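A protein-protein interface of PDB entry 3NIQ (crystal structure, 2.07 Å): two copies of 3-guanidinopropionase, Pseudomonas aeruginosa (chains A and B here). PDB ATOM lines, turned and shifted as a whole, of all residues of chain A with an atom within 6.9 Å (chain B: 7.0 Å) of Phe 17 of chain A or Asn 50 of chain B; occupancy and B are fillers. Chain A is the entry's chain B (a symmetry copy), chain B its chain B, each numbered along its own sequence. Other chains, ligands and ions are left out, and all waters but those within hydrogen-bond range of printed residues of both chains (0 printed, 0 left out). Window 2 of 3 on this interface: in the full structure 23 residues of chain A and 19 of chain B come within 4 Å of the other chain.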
ATOM      1  N   ILE A  14     -17.843  29.760  37.491  1.00  0.00           N
ATOM      2  CA  ILE A  14     -16.764  29.117  36.743  1.00  0.00           C
ATOM      3  C   ILE A  14     -17.369  28.067  35.813  1.00  0.00           C
ATOM      4  O   ILE A  14     -17.869  27.042  36.272  1.00  0.00           O
ATOM      5  CB  ILE A  14     -15.711  28.485  37.672  1.00  0.00           C
ATOM      6  CG1 ILE A  14     -15.253  29.504  38.721  1.00  0.00           C
ATOM      7  CG2 ILE A  14     -14.534  27.928  36.848  1.00  0.00           C
ATOM      8  CD1 ILE A  14     -14.114  29.049  39.611  1.00  0.00           C
ATOM      9  N   PRO A  15     -17.360  28.343  34.496  1.00  0.00           N
ATOM     10  CA  PRO A  15     -17.978  27.442  33.525  1.00  0.00           C
ATOM     11  C   PRO A  15     -17.334  26.058  33.553  1.00  0.00           C
ATOM     12  O   PRO A  15     -16.177  25.923  33.969  1.00  0.00           O
ATOM     13  CB  PRO A  15     -17.724  28.127  32.182  1.00  0.00           C
ATOM     14  CG  PRO A  15     -17.334  29.535  32.502  1.00  0.00           C
ATOM     15  CD  PRO A  15     -16.737  29.522  33.864  1.00  0.00           C
ATOM     16  N   ARG A  16     -18.081  25.046  33.104  1.00  0.00           N
ATOM     17  CA  ARG A  16     -17.691  23.646  33.255  1.00  0.00           C
ATOM     18  C   ARG A  16     -16.467  23.232  32.430  1.00  0.00           C
ATOM     19  O   ARG A  16     -15.848  22.206  32.712  1.00  0.00           O
ATOM     20  CB  ARG A  16     -18.889  22.731  32.957  1.00  0.00           C
ATOM     21  CG  ARG A  16     -20.068  23.018  33.879  1.00  0.00           C
ATOM     22  CD  ARG A  16     -21.168  21.991  33.817  1.00  0.00           C
ATOM     23  NE  ARG A  16     -22.146  22.253  34.881  1.00  0.00           N
ATOM     24  CZ  ARG A  16     -22.051  21.818  36.142  1.00  0.00           C
ATOM     25  NH1 ARG A  16     -21.024  21.065  36.542  1.00  0.00           N
ATOM     26  NH2 ARG A  16     -22.995  22.130  37.018  1.00  0.00           N
ATOM     27  N   PHE A  17     -16.130  24.025  31.418  1.00  0.00           N
ATOM     28  CA  PHE A  17     -14.959  23.768  30.598  1.00  0.00           C
ATOM     29  C   PHE A  17     -13.691  24.328  31.244  1.00  0.00           C
ATOM     30  O   PHE A  17     -12.594  24.127  30.722  1.00  0.00           O
ATOM     31  CB  PHE A  17     -15.138  24.334  29.185  1.00  0.00           C
ATOM     32  CG  PHE A  17     -15.566  25.791  29.141  1.00  0.00           C
ATOM     33  CD1 PHE A  17     -14.649  26.815  29.331  1.00  0.00           C
ATOM     34  CD2 PHE A  17     -16.894  26.129  28.868  1.00  0.00           C
ATOM     35  CE1 PHE A  17     -15.049  28.165  29.273  1.00  0.00           C
ATOM     36  CE2 PHE A  17     -17.308  27.445  28.827  1.00  0.00           C
ATOM     37  CZ  PHE A  17     -16.379  28.482  29.033  1.00  0.00           C
ATOM     38  N   ALA A  18     -13.851  25.027  32.367  1.00  0.00           N
ATOM     39  CA  ALA A  18     -12.754  25.744  33.016  1.00  0.00           C
ATOM     40  C   ALA A  18     -12.401  25.148  34.371  1.00  0.00           C
ATOM     41  O   ALA A  18     -13.142  24.312  34.906  1.00  0.00           O
ATOM     42  CB  ALA A  18     -13.105  27.220  33.188  1.00  0.00           C
ATOM     43  N   GLY A  19     -11.255  25.560  34.910  1.00  0.00           N
ATOM     44  CA  GLY A  19     -10.820  25.076  36.215  1.00  0.00           C
ATOM     45  C   GLY A  19     -10.013  23.806  36.060  1.00  0.00           C
ATOM     46  O   GLY A  19     -10.175  23.061  35.097  1.00  0.00           O
ATOM     47  N   ARG A  25     -14.742  18.375  39.839  1.00  0.00           N
ATOM     48  CA  ARG A  25     -14.146  19.691  40.139  1.00  0.00           C
ATOM     49  C   ARG A  25     -14.127  19.994  41.649  1.00  0.00           C
ATOM     50  O   ARG A  25     -14.296  21.141  42.060  1.00  0.00           O
ATOM     51  CB  ARG A  25     -14.809  20.842  39.343  1.00  0.00           C
ATOM     52  CG  ARG A  25     -14.721  20.667  37.818  1.00  0.00           C
ATOM     53  CD  ARG A  25     -14.903  21.976  37.059  1.00  0.00           C
ATOM     54  NE  ARG A  25     -16.247  22.537  37.241  1.00  0.00           N
ATOM     55  CZ  ARG A  25     -16.587  23.770  36.889  1.00  0.00           C
ATOM     56  NH1 ARG A  25     -15.692  24.565  36.304  1.00  0.00           N
ATOM     57  NH2 ARG A  25     -17.824  24.207  37.106  1.00  0.00           N
ATOM     58  N   SER A  66     -16.541  17.001  34.944  1.00  0.00           N
ATOM     59  CA  SER A  66     -16.858  18.429  34.955  1.00  0.00           C
ATOM     60  C   SER A  66     -18.294  18.703  34.575  1.00  0.00           C
ATOM     61  O   SER A  66     -18.846  19.766  34.893  1.00  0.00           O
ATOM     62  CB  SER A  66     -15.961  19.159  33.940  1.00  0.00           C
ATOM     63  OG  SER A  66     -14.737  19.477  34.566  1.00  0.00           O
ATOM     64  N   LEU A  67     -18.897  17.759  33.871  1.00  0.00           N
ATOM     65  CA  LEU A  67     -20.279  17.922  33.411  1.00  0.00           C
ATOM     66  C   LEU A  67     -21.293  17.607  34.511  1.00  0.00           C
ATOM     67  O   LEU A  67     -22.467  17.931  34.377  1.00  0.00           O
ATOM     68  CB  LEU A  67     -20.530  17.042  32.179  1.00  0.00           C
ATOM     69  CG  LEU A  67     -19.650  17.345  30.963  1.00  0.00           C
ATOM     70  CD1 LEU A  67     -20.124  16.541  29.729  1.00  0.00           C
ATOM     71  CD2 LEU A  67     -19.692  18.825  30.677  1.00  0.00           C
ATOM     72  N   GLY B  47     -25.825  31.565  22.797  1.00  0.00           N
ATOM     73  CA  GLY B  47     -26.436  31.232  24.091  1.00  0.00           C
ATOM     74  C   GLY B  47     -25.786  30.086  24.853  1.00  0.00           C
ATOM     75  O   GLY B  47     -26.234  29.722  25.955  1.00  0.00           O
ATOM     76  N   THR B  48     -24.732  29.495  24.282  1.00  0.00           N
ATOM     77  CA  THR B  48     -24.186  28.247  24.832  1.00  0.00           C
ATOM     78  C   THR B  48     -23.217  28.482  25.992  1.00  0.00           C
ATOM     79  O   THR B  48     -22.218  29.185  25.848  1.00  0.00           O
ATOM     80  CB  THR B  48     -23.526  27.382  23.722  1.00  0.00           C
ATOM     81  OG1 THR B  48     -24.548  26.842  22.861  1.00  0.00           O
ATOM     82  CG2 THR B  48     -22.763  26.264  24.340  1.00  0.00           C
ATOM     83  N   THR B  49     -23.493  27.834  27.120  1.00  0.00           N
ATOM     84  CA  THR B  49     -22.750  28.063  28.354  1.00  0.00           C
ATOM     85  C   THR B  49     -21.608  27.054  28.568  1.00  0.00           C
ATOM     86  O   THR B  49     -20.706  27.304  29.372  1.00  0.00           O
ATOM     87  CB  THR B  49     -23.701  27.975  29.563  1.00  0.00           C
ATOM     88  OG1 THR B  49     -24.250  26.649  29.615  1.00  0.00           O
ATOM     89  CG2 THR B  49     -24.841  28.981  29.417  1.00  0.00           C
ATOM     90  N   ASN B  50     -21.661  25.923  27.854  1.00  0.00           N
ATOM     91  CA  ASN B  50     -20.628  24.893  27.940  1.00  0.00           C
ATOM     92  C   ASN B  50     -19.957  24.645  26.578  1.00  0.00           C
ATOM     93  O   ASN B  50     -19.090  25.420  26.169  1.00  0.00           O
ATOM     94  CB  ASN B  50     -21.178  23.591  28.570  1.00  0.00           C
ATOM     95  CG  ASN B  50     -20.093  22.507  28.767  1.00  0.00           C
ATOM     96  OD1 ASN B  50     -20.349  21.318  28.549  1.00  0.00           O
ATOM     97  ND2 ASN B  50     -18.881  22.923  29.140  1.00  0.00           N
ATOM     98  N   ARG B  51     -20.349  23.582  25.875  1.00  0.00           N
ATOM     99  CA  ARG B  51     -19.700  23.266  24.589  1.00  0.00           C
ATOM    100  C   ARG B  51     -20.437  23.931  23.446  1.00  0.00           C
ATOM    101  O   ARG B  51     -21.633  23.696  23.247  1.00  0.00           O
ATOM    102  CB  ARG B  51     -19.581  21.752  24.377  1.00  0.00           C
ATOM    103  CG  ARG B  51     -18.987  21.041  25.612  1.00  0.00           C
ATOM    104  CD  ARG B  51     -18.508  19.634  25.332  1.00  0.00           C
ATOM    105  NE  ARG B  51     -19.556  18.775  24.797  1.00  0.00           N
ATOM    106  CZ  ARG B  51     -19.446  17.454  24.653  1.00  0.00           C
ATOM    107  NH1 ARG B  51     -18.344  16.823  25.025  1.00  0.00           N
ATOM    108  NH2 ARG B  51     -20.451  16.761  24.140  1.00  0.00           N
ATOM    109  N   ALA B  52     -19.735  24.795  22.717  1.00  0.00           N
ATOM    110  CA  ALA B  52     -20.339  25.457  21.573  1.00  0.00           C
ATOM    111  C   ALA B  52     -20.141  24.584  20.319  1.00  0.00           C
ATOM    112  O   ALA B  52     -19.592  23.486  20.408  1.00  0.00           O
ATOM    113  CB  ALA B  52     -19.745  26.836  21.390  1.00  0.00           C
ATOM    114  N   PHE B 158     -24.224  33.122  35.063  1.00  0.00           N
ATOM    115  CA  PHE B 158     -22.981  33.873  35.327  1.00  0.00           C
ATOM    116  C   PHE B 158     -23.237  35.368  35.494  1.00  0.00           C
ATOM    117  O   PHE B 158     -22.657  36.193  34.786  1.00  0.00           O
ATOM    118  CB  PHE B 158     -21.935  33.642  34.213  1.00  0.00           C
ATOM    119  CG  PHE B 158     -21.787  32.198  33.780  1.00  0.00           C
ATOM    120  CD1 PHE B 158     -21.040  31.295  34.535  1.00  0.00           C
ATOM    121  CD2 PHE B 158     -22.364  31.754  32.585  1.00  0.00           C
ATOM    122  CE1 PHE B 158     -20.904  29.957  34.116  1.00  0.00           C
ATOM    123  CE2 PHE B 158     -22.235  30.435  32.158  1.00  0.00           C
ATOM    124  CZ  PHE B 158     -21.508  29.528  32.917  1.00  0.00           C
ATOM    125  N   HIS B 165     -29.078  29.350  26.167  1.00  0.00           N
ATOM    126  CA  HIS B 165     -29.817  28.180  25.690  1.00  0.00           C
ATOM    127  C   HIS B 165     -30.580  27.490  26.834  1.00  0.00           C
ATOM    128  O   HIS B 165     -31.430  26.624  26.595  1.00  0.00           O
ATOM    129  CB  HIS B 165     -28.886  27.202  24.950  1.00  0.00           C
ATOM    130  CG  HIS B 165     -27.811  26.598  25.805  1.00  0.00           C
ATOM    131  ND1 HIS B 165     -27.204  25.398  25.488  1.00  0.00           N
ATOM    132  CD2 HIS B 165     -27.224  27.026  26.953  1.00  0.00           C
ATOM    133  CE1 HIS B 165     -26.285  25.117  26.402  1.00  0.00           C
ATOM    134  NE2 HIS B 165     -26.280  26.088  27.302  1.00  0.00           N
ATOM    135  N   GLY B 253     -24.091  19.745  22.697  1.00  0.00           N
ATOM    136  CA  GLY B 253     -23.328  20.498  23.669  1.00  0.00           C
ATOM    137  C   GLY B 253     -23.437  20.018  25.096  1.00  0.00           C
ATOM    138  O   GLY B 253     -22.434  20.045  25.817  1.00  0.00           O
ATOM    139  N   THR B 254     -24.638  19.576  25.499  1.00  0.00           N
ATOM    140  CA  THR B 254     -24.903  19.190  26.893  1.00  0.00           C
ATOM    141  C   THR B 254     -25.508  17.779  26.991  1.00  0.00           C
ATOM    142  O   THR B 254     -26.690  17.610  27.310  1.00  0.00           O
ATOM    143  CB  THR B 254     -25.830  20.217  27.585  1.00  0.00           C
ATOM    144  OG1 THR B 254     -25.278  21.530  27.442  1.00  0.00           O
ATOM    145  CG2 THR B 254     -25.951  19.900  29.079  1.00  0.00           C
ATOM    146  N   PRO B 255     -24.702  16.753  26.702  1.00  0.00           N
ATOM    147  CA  PRO B 255     -25.192  15.394  26.762  1.00  0.00           C
ATOM    148  C   PRO B 255     -25.539  14.955  28.185  1.00  0.00           C
ATOM    149  O   PRO B 255     -24.903  15.405  29.144  1.00  0.00           O
ATOM    150  CB  PRO B 255     -23.995  14.575  26.247  1.00  0.00           C
ATOM    151  CG  PRO B 255     -22.828  15.386  26.562  1.00  0.00           C
ATOM    152  CD  PRO B 255     -23.251  16.809  26.442  1.00  0.00           C
ATOM    153  N   PHE B 289     -18.803  17.968  17.655  1.00  0.00           N
ATOM    154  CA  PHE B 289     -18.830  16.861  18.611  1.00  0.00           C
ATOM    155  C   PHE B 289     -19.488  15.638  18.036  1.00  0.00           C
ATOM    156  O   PHE B 289     -19.724  14.674  18.748  1.00  0.00           O
ATOM    157  CB  PHE B 289     -19.480  17.280  19.936  1.00  0.00           C
ATOM    158  CG  PHE B 289     -18.684  18.309  20.665  1.00  0.00           C
ATOM    159  CD1 PHE B 289     -17.535  17.941  21.375  1.00  0.00           C
ATOM    160  CD2 PHE B 289     -19.035  19.634  20.606  1.00  0.00           C
ATOM    161  CE1 PHE B 289     -16.759  18.892  22.010  1.00  0.00           C
ATOM    162  CE2 PHE B 289     -18.269  20.592  21.232  1.00  0.00           C
ATOM    163  CZ  PHE B 289     -17.122  20.223  21.935  1.00  0.00           C
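The side-chain hydroxyl of Thr 49 of chain B is in hydrogen-bond range of a ring nitrogen (NE2) of His 165 of chain B, 3.1 Å away.
The guanidinium group (NH1) of Arg 25 of chain A sits at hydrogen-bond distance from the backbone carbonyl oxygen (O) of Pro 15 of chain A.
The guanidinium group (NH1) of Arg 16 of chain A is in hydrogen-bond range of the backbone carbonyl oxygen (O) of Ser 66 of chain A (3.0 Å).
Among the printed residues, merely in contact across the chains: Pro 15 of chain A with Phe 158 of chain B, Arg 16 of chain A with Asn 50 of chain B, Phe 17 of chain A with Thr 49 of chain B, Phe 17 of chain A with Asn 50 of chain B and Leu 67 of chain A with Asn 50 of chain B.
Of chain A, only Arg 16 (3.8 Å), Phe 17 (3.6 Å) and Leu 67 (3.3 Å) come within 4 Å of Asn 50 of chain B.
Of the printed residues of chain B, Leu 67 of chain A touches Asn 50.
Of the printed residues of chain A, Phe 158 of chain B touches Pro 15 (3.9 Å).
Thr 254 of chain B touches none of the printed residues of chain A.
Gly 19 of chain A touches none of the printed residues of chain B.
The nearest printed residue of chain B that does not touch Pro 15 of chain A is Thr 49 of chain B (4.2 Å).
Of the 12 printed residues of chain B, 3 touch a printed residue of chain A.
Hydrophobic or aromatic side chains of chain B within 4 Å of the printed part of chain A: Phe 158.
Of the 9 printed residues of chain A, 4 touch a printed residue of chain B.
Hydrophobic or aromatic side chains of chain A within 4 Å of the printed part of chain B: Pro 15, Phe 17 and Leu 67.
Among the printed residues, no Asp or Glu carboxylate lies within 4 Å of a Lys or Arg side-chain nitrogen of the other chain.
No position is printed for both chains.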
